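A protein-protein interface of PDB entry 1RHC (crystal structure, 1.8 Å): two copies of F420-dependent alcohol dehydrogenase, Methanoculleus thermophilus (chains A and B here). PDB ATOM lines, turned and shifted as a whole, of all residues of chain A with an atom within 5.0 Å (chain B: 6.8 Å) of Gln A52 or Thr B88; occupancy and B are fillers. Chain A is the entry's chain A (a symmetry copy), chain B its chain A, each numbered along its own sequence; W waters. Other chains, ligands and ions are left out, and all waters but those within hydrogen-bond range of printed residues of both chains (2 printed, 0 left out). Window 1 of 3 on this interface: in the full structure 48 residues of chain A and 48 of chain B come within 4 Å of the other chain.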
ATOM      1  N   LEU A  11      26.305  24.680  30.519  1.00  0.00           N
ATOM      2  CA  LEU A  11      26.783  24.626  29.143  1.00  0.00           C
ATOM      3  C   LEU A  11      27.939  25.619  28.977  1.00  0.00           C
ATOM      4  O   LEU A  11      28.375  25.879  27.871  1.00  0.00           O
ATOM      5  CB  LEU A  11      25.636  24.988  28.177  1.00  0.00           C
ATOM      6  CG  LEU A  11      24.438  24.025  28.303  1.00  0.00           C
ATOM      7  CD1 LEU A  11      23.378  24.422  27.252  1.00  0.00           C
ATOM      8  CD2 LEU A  11      24.852  22.552  28.104  1.00  0.00           C
ATOM      9  N   ASP A  38      21.679  29.889  29.761  1.00  0.00           N
ATOM     10  CA  ASP A  38      21.433  30.281  28.366  1.00  0.00           C
ATOM     11  C   ASP A  38      22.352  31.460  28.070  1.00  0.00           C
ATOM     12  O   ASP A  38      22.014  32.615  28.303  1.00  0.00           O
ATOM     13  CB  ASP A  38      19.948  30.660  28.226  1.00  0.00           C
ATOM     14  CG  ASP A  38      19.522  30.834  26.795  1.00  0.00           C
ATOM     15  OD1 ASP A  38      20.381  31.053  25.900  1.00  0.00           O
ATOM     16  OD2 ASP A  38      18.300  30.789  26.579  1.00  0.00           O
ATOM     17  N   SER A  50      30.169  27.599  25.599  1.00  0.00           N
ATOM     18  CA  SER A  50      28.918  28.373  25.693  1.00  0.00           C
ATOM     19  C   SER A  50      28.002  27.761  24.657  1.00  0.00           C
ATOM     20  O   SER A  50      27.841  28.318  23.569  1.00  0.00           O
ATOM     21  CB  SER A  50      29.110  29.863  25.387  1.00  0.00           C
ATOM     22  OG  SER A  50      29.075  30.585  26.601  1.00  0.00           O
ATOM     23  N   ALA A  51      27.417  26.618  24.994  1.00  0.00           N
ATOM     24  CA  ALA A  51      26.543  25.899  24.032  1.00  0.00           C
ATOM     25  C   ALA A  51      25.144  26.534  24.017  1.00  0.00           C
ATOM     26  O   ALA A  51      24.714  27.148  25.010  1.00  0.00           O
ATOM     27  CB  ALA A  51      26.460  24.433  24.428  1.00  0.00           C
ATOM     28  N   GLN A  52      24.434  26.396  22.900  1.00  0.00           N
ATOM     29  CA  GLN A  52      23.108  27.016  22.776  1.00  0.00           C
ATOM     30  C   GLN A  52      22.088  26.151  23.519  1.00  0.00           C
ATOM     31  O   GLN A  52      21.908  24.957  23.241  1.00  0.00           O
ATOM     32  CB  GLN A  52      22.768  27.202  21.297  1.00  0.00           C
ATOM     33  CG  GLN A  52      21.813  28.379  21.051  1.00  0.00           C
ATOM     34  CD  GLN A  52      20.371  28.051  21.436  1.00  0.00           C
ATOM     35  OE1 GLN A  52      19.921  26.939  21.239  1.00  0.00           O
ATOM     36  NE2 GLN A  52      19.644  29.029  21.940  1.00  0.00           N
ATOM     37  N   ALA A  53      21.418  26.779  24.467  1.00  0.00           N
ATOM     38  CA  ALA A  53      20.548  26.057  25.381  1.00  0.00           C
ATOM     39  C   ALA A  53      19.282  25.429  24.851  1.00  0.00           C
ATOM     40  O   ALA A  53      18.850  24.406  25.368  1.00  0.00           O
ATOM     41  CB  ALA A  53      20.219  26.971  26.581  1.00  0.00           C
ATOM     42  N   TRP A  54      18.657  26.048  23.844  1.00  0.00           N
ATOM     43  CA  TRP A  54      17.388  25.527  23.349  1.00  0.00           C
ATOM     44  C   TRP A  54      17.580  24.234  22.584  1.00  0.00           C
ATOM     45  O   TRP A  54      16.795  23.298  22.733  1.00  0.00           O
ATOM     46  CB  TRP A  54      16.731  26.551  22.440  1.00  0.00           C
ATOM     47  CG  TRP A  54      16.636  27.951  23.001  1.00  0.00           C
ATOM     48  CD1 TRP A  54      16.933  28.388  24.267  1.00  0.00           C
ATOM     49  CD2 TRP A  54      16.161  29.075  22.287  1.00  0.00           C
ATOM     50  NE1 TRP A  54      16.656  29.747  24.378  1.00  0.00           N
ATOM     51  CE2 TRP A  54      16.185  30.182  23.164  1.00  0.00           C
ATOM     52  CE3 TRP A  54      15.719  29.256  20.967  1.00  0.00           C
ATOM     53  CZ2 TRP A  54      15.777  31.456  22.769  1.00  0.00           C
ATOM     54  CZ3 TRP A  54      15.318  30.527  20.576  1.00  0.00           C
ATOM     55  CH2 TRP A  54      15.352  31.610  21.474  1.00  0.00           C
ATOM     56  N   ALA A  55      18.610  24.194  21.744  1.00  0.00           N
ATOM     57  CA  ALA A  55      18.933  22.982  20.985  1.00  0.00           C
ATOM     58  C   ALA A  55      19.296  21.884  21.989  1.00  0.00           C
ATOM     59  O   ALA A  55      18.837  20.746  21.867  1.00  0.00           O
ATOM     60  CB  ALA A  55      20.121  23.261  20.030  1.00  0.00           C
ATOM     61  N   TRP A  56      20.088  22.226  23.000  1.00  0.00           N
ATOM     62  CA  TRP A  56      20.492  21.246  24.026  1.00  0.00           C
ATOM     63  C   TRP A  56      19.246  20.719  24.767  1.00  0.00           C
ATOM     64  O   TRP A  56      19.142  19.523  25.078  1.00  0.00           O
ATOM     65  CB  TRP A  56      21.442  21.910  25.032  1.00  0.00           C
ATOM     66  CG  TRP A  56      21.953  20.950  26.097  1.00  0.00           C
ATOM     67  CD1 TRP A  56      23.098  20.150  26.041  1.00  0.00           C
ATOM     68  CD2 TRP A  56      21.347  20.686  27.365  1.00  0.00           C
ATOM     69  NE1 TRP A  56      23.227  19.433  27.216  1.00  0.00           N
ATOM     70  CE2 TRP A  56      22.173  19.740  28.042  1.00  0.00           C
ATOM     71  CE3 TRP A  56      20.190  21.160  28.007  1.00  0.00           C
ATOM     72  CZ2 TRP A  56      21.870  19.267  29.320  1.00  0.00           C
ATOM     73  CZ3 TRP A  56      19.894  20.684  29.277  1.00  0.00           C
ATOM     74  CH2 TRP A  56      20.732  19.748  29.923  1.00  0.00           C
ATOM     75  N   TYR A  80      17.672  37.630  21.480  1.00  0.00           N
ATOM     76  CA  TYR A  80      16.525  36.739  21.211  1.00  0.00           C
ATOM     77  C   TYR A  80      15.272  37.624  21.083  1.00  0.00           C
ATOM     78  O   TYR A  80      15.132  38.610  21.806  1.00  0.00           O
ATOM     79  CB  TYR A  80      16.244  35.773  22.352  1.00  0.00           C
ATOM     80  CG  TYR A  80      17.336  34.739  22.618  1.00  0.00           C
ATOM     81  CD1 TYR A  80      17.912  34.014  21.575  1.00  0.00           C
ATOM     82  CD2 TYR A  80      17.703  34.427  23.929  1.00  0.00           C
ATOM     83  CE1 TYR A  80      18.820  32.981  21.838  1.00  0.00           C
ATOM     84  CE2 TYR A  80      18.622  33.408  24.205  1.00  0.00           C
ATOM     85  CZ  TYR A  80      19.164  32.684  23.141  1.00  0.00           C
ATOM     86  OH  TYR A  80      20.027  31.624  23.384  1.00  0.00           O
ATOM     87  N   TRP B  54      14.764  24.423  15.892  1.00  0.00           N
ATOM     88  CA  TRP B  54      16.037  24.149  16.546  1.00  0.00           C
ATOM     89  C   TRP B  54      15.858  23.251  17.753  1.00  0.00           C
ATOM     90  O   TRP B  54      16.654  22.339  17.976  1.00  0.00           O
ATOM     91  CB  TRP B  54      16.682  25.452  16.986  1.00  0.00           C
ATOM     92  CG  TRP B  54      16.761  26.527  15.926  1.00  0.00           C
ATOM     93  CD1 TRP B  54      16.463  26.435  14.591  1.00  0.00           C
ATOM     94  CD2 TRP B  54      17.223  27.844  16.149  1.00  0.00           C
ATOM     95  NE1 TRP B  54      16.724  27.649  13.963  1.00  0.00           N
ATOM     96  CE2 TRP B  54      17.189  28.525  14.912  1.00  0.00           C
ATOM     97  CE3 TRP B  54      17.660  28.528  17.296  1.00  0.00           C
ATOM     98  CZ2 TRP B  54      17.582  29.857  14.782  1.00  0.00           C
ATOM     99  CZ3 TRP B  54      18.047  29.855  17.163  1.00  0.00           C
ATOM    100  CH2 TRP B  54      18.002  30.506  15.915  1.00  0.00           C
ATOM    101  N   ALA B  55      14.827  23.528  18.545  1.00  0.00           N
ATOM    102  CA  ALA B  55      14.516  22.701  19.715  1.00  0.00           C
ATOM    103  C   ALA B  55      14.168  21.295  19.216  1.00  0.00           C
ATOM    104  O   ALA B  55      14.639  20.298  19.768  1.00  0.00           O
ATOM    105  CB  ALA B  55      13.321  23.314  20.490  1.00  0.00           C
ATOM    106  N   ALA B  83      24.343  35.483  14.436  1.00  0.00           N
ATOM    107  CA  ALA B  83      25.359  34.946  15.336  1.00  0.00           C
ATOM    108  C   ALA B  83      24.742  33.816  16.179  1.00  0.00           C
ATOM    109  O   ALA B  83      25.420  32.844  16.528  1.00  0.00           O
ATOM    110  CB  ALA B  83      25.866  36.075  16.252  1.00  0.00           C
ATOM    111  N   ILE B  84      23.469  33.976  16.555  1.00  0.00           N
ATOM    112  CA  ILE B  84      22.771  32.947  17.322  1.00  0.00           C
ATOM    113  C   ILE B  84      22.530  31.714  16.437  1.00  0.00           C
ATOM    114  O   ILE B  84      22.611  30.582  16.916  1.00  0.00           O
ATOM    115  CB  ILE B  84      21.418  33.460  17.874  1.00  0.00           C
ATOM    116  CG1 ILE B  84      21.633  34.689  18.777  1.00  0.00           C
ATOM    117  CG2 ILE B  84      20.710  32.353  18.614  1.00  0.00           C
ATOM    118  CD1 ILE B  84      22.620  34.488  19.906  1.00  0.00           C
ATOM    119  N   VAL B  85      22.229  31.913  15.155  1.00  0.00           N
ATOM    120  CA  VAL B  85      22.077  30.778  14.247  1.00  0.00           C
ATOM    121  C   VAL B  85      23.414  30.057  14.164  1.00  0.00           C
ATOM    122  O   VAL B  85      23.483  28.824  14.206  1.00  0.00           O
ATOM    123  CB  VAL B  85      21.658  31.236  12.816  1.00  0.00           C
ATOM    124  CG1 VAL B  85      21.590  30.024  11.881  1.00  0.00           C
ATOM    125  CG2 VAL B  85      20.257  31.949  12.864  1.00  0.00           C
ATOM    126  N   ALA B  86      24.500  30.821  14.059  1.00  0.00           N
ATOM    127  CA  ALA B  86      25.808  30.203  14.003  1.00  0.00           C
ATOM    128  C   ALA B  86      26.087  29.371  15.255  1.00  0.00           C
ATOM    129  O   ALA B  86      26.609  28.256  15.163  1.00  0.00           O
ATOM    130  CB  ALA B  86      26.898  31.279  13.814  1.00  0.00           C
ATOM    131  N   GLN B  87      25.732  29.904  16.423  1.00  0.00           N
ATOM    132  CA  GLN B  87      25.960  29.199  17.682  1.00  0.00           C
ATOM    133  C   GLN B  87      25.121  27.910  17.769  1.00  0.00           C
ATOM    134  O   GLN B  87      25.601  26.868  18.197  1.00  0.00           O
ATOM    135  CB  GLN B  87      25.567  30.101  18.856  1.00  0.00           C
ATOM    136  CG  GLN B  87      25.952  29.515  20.233  1.00  0.00           C
ATOM    137  CD  GLN B  87      25.271  30.219  21.407  1.00  0.00           C
ATOM    138  OE1 GLN B  87      25.564  29.912  22.577  1.00  0.00           O
ATOM    139  NE2 GLN B  87      24.345  31.139  21.119  1.00  0.00           N
ATOM    140  N   THR B  88      23.857  28.007  17.381  1.00  0.00           N
ATOM    141  CA  THR B  88      22.965  26.854  17.473  1.00  0.00           C
ATOM    142  C   THR B  88      23.476  25.635  16.707  1.00  0.00           C
ATOM    143  O   THR B  88      23.553  24.520  17.260  1.00  0.00           O
ATOM    144  CB  THR B  88      21.553  27.241  16.968  1.00  0.00           C
ATOM    145  OG1 THR B  88      21.049  28.312  17.790  1.00  0.00           O
ATOM    146  CG2 THR B  88      20.610  26.029  17.021  1.00  0.00           C
ATOM    147  N   PHE B  89      23.870  25.838  15.454  1.00  0.00           N
ATOM    148  CA  PHE B  89      24.316  24.705  14.652  1.00  0.00           C
ATOM    149  C   PHE B  89      25.713  24.248  14.980  1.00  0.00           C
ATOM    150  O   PHE B  89      26.015  23.085  14.844  1.00  0.00           O
ATOM    151  CB  PHE B  89      24.077  25.020  13.162  1.00  0.00           C
ATOM    152  CG  PHE B  89      22.605  25.109  12.844  1.00  0.00           C
ATOM    153  CD1 PHE B  89      21.911  26.307  12.989  1.00  0.00           C
ATOM    154  CD2 PHE B  89      21.877  23.948  12.565  1.00  0.00           C
ATOM    155  CE1 PHE B  89      20.523  26.364  12.879  1.00  0.00           C
ATOM    156  CE2 PHE B  89      20.478  23.987  12.448  1.00  0.00           C
ATOM    157  CZ  PHE B  89      19.801  25.186  12.609  1.00  0.00           C
ATOM    158  N   ALA B  90      26.566  25.154  15.450  1.00  0.00           N
ATOM    159  CA  ALA B  90      27.898  24.720  15.907  1.00  0.00           C
ATOM    160  C   ALA B  90      27.708  23.825  17.164  1.00  0.00           C
ATOM    161  O   ALA B  90      28.385  22.812  17.351  1.00  0.00           O
ATOM    162  CB  ALA B  90      28.774  25.967  16.259  1.00  0.00           C
ATOM    163  N   THR B  91      26.789  24.210  18.044  1.00  0.00           N
ATOM    164  CA  THR B  91      26.523  23.419  19.235  1.00  0.00           C
ATOM    165  C   THR B  91      26.012  22.015  18.858  1.00  0.00           C
ATOM    166  O   THR B  91      26.517  21.012  19.356  1.00  0.00           O
ATOM    167  CB  THR B  91      25.485  24.094  20.156  1.00  0.00           C
ATOM    168  OG1 THR B  91      26.099  25.200  20.831  1.00  0.00           O
ATOM    169  CG2 THR B  91      24.959  23.102  21.219  1.00  0.00           C
ATOM    170  N   LEU B  92      25.026  21.944  17.961  1.00  0.00           N
ATOM    171  CA  LEU B  92      24.473  20.637  17.601  1.00  0.00           C
ATOM    172  C   LEU B  92      25.520  19.771  16.895  1.00  0.00           C
ATOM    173  O   LEU B  92      25.606  18.555  17.133  1.00  0.00           O
ATOM    174  CB  LEU B  92      23.243  20.831  16.704  1.00  0.00           C
ATOM    175  CG  LEU B  92      22.027  21.298  17.508  1.00  0.00           C
ATOM    176  CD1 LEU B  92      20.892  21.635  16.538  1.00  0.00           C
ATOM    177  CD2 LEU B  92      21.577  20.197  18.484  1.00  0.00           C
ATOM    178  N   ARG B  93      26.323  20.376  16.032  1.00  0.00           N
ATOM    179  CA  ARG B  93      27.358  19.581  15.370  1.00  0.00           C
ATOM    180  C   ARG B  93      28.440  19.128  16.349  1.00  0.00           C
ATOM    181  O   ARG B  93      29.040  18.057  16.154  1.00  0.00           O
ATOM    182  CB  ARG B  93      27.961  20.348  14.191  1.00  0.00           C
ATOM    183  CG  ARG B  93      28.757  19.422  13.222  1.00  0.00           C
ATOM    184  CD  ARG B  93      29.084  20.117  11.899  1.00  0.00           C
ATOM    185  NE  ARG B  93      30.027  19.327  11.072  1.00  0.00           N
ATOM    186  CZ  ARG B  93      29.672  18.435  10.165  1.00  0.00           C
ATOM    187  NH1 ARG B  93      30.626  17.798   9.492  1.00  0.00           N
ATOM    188  NH2 ARG B  93      28.377  18.167   9.909  1.00  0.00           N
ATOM    189  N   MET B  95      27.825  18.246  19.431  1.00  0.00           N
ATOM    190  CA  MET B  95      27.149  17.128  20.109  1.00  0.00           C
ATOM    191  C   MET B  95      26.982  15.867  19.259  1.00  0.00           C
ATOM    192  O   MET B  95      27.082  14.750  19.780  1.00  0.00           O
ATOM    193  CB  MET B  95      25.757  17.578  20.590  1.00  0.00           C
ATOM    194  CG  MET B  95      25.837  18.530  21.789  1.00  0.00           C
ATOM    195  SD  MET B  95      24.167  19.180  22.189  1.00  0.00           S
ATOM    196  CE  MET B  95      23.501  17.829  23.065  1.00  0.00           C
ATOM    197  N   VAL B 100      25.207  17.158  11.313  1.00  0.00           N
ATOM    198  CA  VAL B 100      24.436  18.414  11.343  1.00  0.00           C
ATOM    199  C   VAL B 100      24.804  19.426  10.279  1.00  0.00           C
ATOM    200  O   VAL B 100      25.984  19.694  10.061  1.00  0.00           O
ATOM    201  CB  VAL B 100      24.635  19.107  12.716  1.00  0.00           C
ATOM    202  CG1 VAL B 100      23.875  20.442  12.773  1.00  0.00           C
ATOM    203  CG2 VAL B 100      24.145  18.168  13.836  1.00  0.00           C
ATOM    204  N   TRP B 140      32.287  30.755  12.845  1.00  0.00           N
ATOM    205  CA  TRP B 140      32.658  29.347  12.781  1.00  0.00           C
ATOM    206  C   TRP B 140      34.150  29.113  12.559  1.00  0.00           C
ATOM    207  O   TRP B 140      34.745  28.145  13.075  1.00  0.00           O
ATOM    208  CB  TRP B 140      31.944  28.678  11.632  1.00  0.00           C
ATOM    209  CG  TRP B 140      30.512  28.421  11.894  1.00  0.00           C
ATOM    210  CD1 TRP B 140      29.896  28.292  13.119  1.00  0.00           C
ATOM    211  CD2 TRP B 140      29.515  28.175  10.903  1.00  0.00           C
ATOM    212  NE1 TRP B 140      28.558  27.977  12.932  1.00  0.00           N
ATOM    213  CE2 TRP B 140      28.299  27.900  11.588  1.00  0.00           C
ATOM    214  CE3 TRP B 140      29.526  28.160   9.499  1.00  0.00           C
ATOM    215  CZ2 TRP B 140      27.107  27.612  10.910  1.00  0.00           C
ATOM    216  CZ3 TRP B 140      28.333  27.865   8.823  1.00  0.00           C
ATOM    217  CH2 TRP B 140      27.142  27.595   9.543  1.00  0.00           C
ATOM    218  N   LEU B 160      32.986  32.069  19.322  1.00  0.00           N
ATOM    219  CA  LEU B 160      32.210  30.861  19.599  1.00  0.00           C
ATOM    220  C   LEU B 160      33.065  29.895  20.414  1.00  0.00           C
ATOM    221  O   LEU B 160      33.960  29.229  19.874  1.00  0.00           O
ATOM    222  CB  LEU B 160      31.781  30.142  18.321  1.00  0.00           C
ATOM    223  CG  LEU B 160      30.641  30.664  17.475  1.00  0.00           C
ATOM    224  CD1 LEU B 160      30.323  29.555  16.475  1.00  0.00           C
ATOM    225  CD2 LEU B 160      29.418  30.992  18.327  1.00  0.00           C
ATOM    226  N   THR B 162      32.017  27.162  21.768  1.00  0.00           N
ATOM    227  CA  THR B 162      31.614  25.795  21.478  1.00  0.00           C
ATOM    228  C   THR B 162      31.623  25.593  19.987  1.00  0.00           C
ATOM    229  O   THR B 162      30.737  26.059  19.286  1.00  0.00           O
ATOM    230  CB  THR B 162      30.204  25.507  22.044  1.00  0.00           C
ATOM    231  OG1 THR B 162      30.281  25.528  23.465  1.00  0.00           O
ATOM    232  CG2 THR B 162      29.683  24.138  21.594  1.00  0.00           C
HETATM  233  O   HOH W   1      22.695  32.449  22.771  1.00  0.00           O
HETATM  234  O   HOH W   2      29.619  29.003  21.502  1.00  0.00           O
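The side-chain hydroxyl (OG1) of Thr B91 lies within hydrogen-bond range of the backbone NH (N) of Gln A52, 2.9 Å away.
The side-chain hydroxyl (OG1) of Thr B162 lies within hydrogen-bond range of the backbone NH (N) of Ser A50 (3.0 Å).
The backbone NH (N) of Ala A51 is in hydrogen-bond range of the side-chain hydroxyl (OG1) of Thr B162 (3.4 Å).
The side-chain amide oxygen (OE1) of Gln B87 sits close to the backbone carbonyl oxygen (O) of Ser A50, at 3.0 Å.
The backbone carbonyl oxygen (O) of Ile B84 lies within hydrogen-bond range of the side-chain hydroxyl (OG1) of Thr B88.
The indole nitrogen (NE1) of Trp A54 sits at hydrogen-bond distance from the side-chain carboxylate (OD2) of Asp A38 (2.9 Å).
The side-chain amide oxygen (OE1) of Gln A52 lies within hydrogen-bond range of the backbone NH (N) of Trp A54 (3.0 Å).
O of Leu A11 sits close to N of Ser A50, at 3.4 Å.
The side-chain hydroxyl (OH) of Tyr A80 is in hydrogen-bond range of the side-chain carboxylate (OD1) of Asp A38 (2.6 Å).
The side-chain hydroxyl of Tyr A80 is in hydrogen-bond range of the side-chain amide nitrogen of Gln A52, 3.0 Å away.
Among the printed residues, merely in contact across the chains: Ala A51 with Thr B91 (3.3 Å), Gln A52 with Thr B88 (3.3 Å), Ala A51 with Gln B87 (3.7 Å), Gln A52 with Gln B87 (3.7 Å), Ala A55 with Leu B92 (3.7 Å), Tyr A80 with Ile B84 (3.8 Å), Trp A56 with Met B95 (3.8 Å), Trp A54 with Ala B55 (3.8 Å) and Ala A55 with Trp B54 (3.8 Å).
Gln A52 touches just these residues of chain B: Gln B87, Thr B88 and Thr B91.
Thr B88 touches just one residue of chain A: Gln A52 (3.3 Å).
Of the printed residues of chain A, Met B95 touches Trp A56.
Of the printed residues of chain A, Thr B91 touches Ala A51 and Gln A52.
Of the printed residues of chain B, Trp A54 touches Ala B55 (3.8 Å).
Val B85 touches none of the printed residues of chain A.
Ala B86 touches none of the printed residues of chain A.
The nearest residue of chain B that does not touch Gln A52 is Ile B84 (4.8 Å).
The nearest residue of chain A that does not touch Thr B88 is Ala A55 (4.1 Å).
Hydrophobic or aromatic side chains of chain A that line the printed part of chain B: Ala A51, Ala A55, Trp A56 and Tyr A80.
Along chain A the printed residues that touch a printed residue of chain B span positions 50 to 80.
Of the 18 printed residues of chain B, 9 touch a printed residue of chain A.
Among the printed residues, no Asp or Glu carboxylate lies within 4 Å of a Lys or Arg side-chain nitrogen of the other chain.
Trp A54 touches Ala B55, and with the chains exchanged Ala A55 touches Trp B54.
Positions printed for both chains: 54 and 55.
Of the 13 pairs that touch across the chains among the printed residues, 2 have their exchanged pair printed and touching as well.
Water W1 lies within hydrogen-bond range of the side-chain amide nitrogen of Gln B87 (2.7 Å) and the side-chain hydroxyl of Tyr A80 (2.9 Å).
Water W2 lies within hydrogen-bond range of the backbone carbonyl oxygen (O) of Ser A50 (2.8 Å) and the backbone NH (N) of Thr B162 (3.0 Å).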
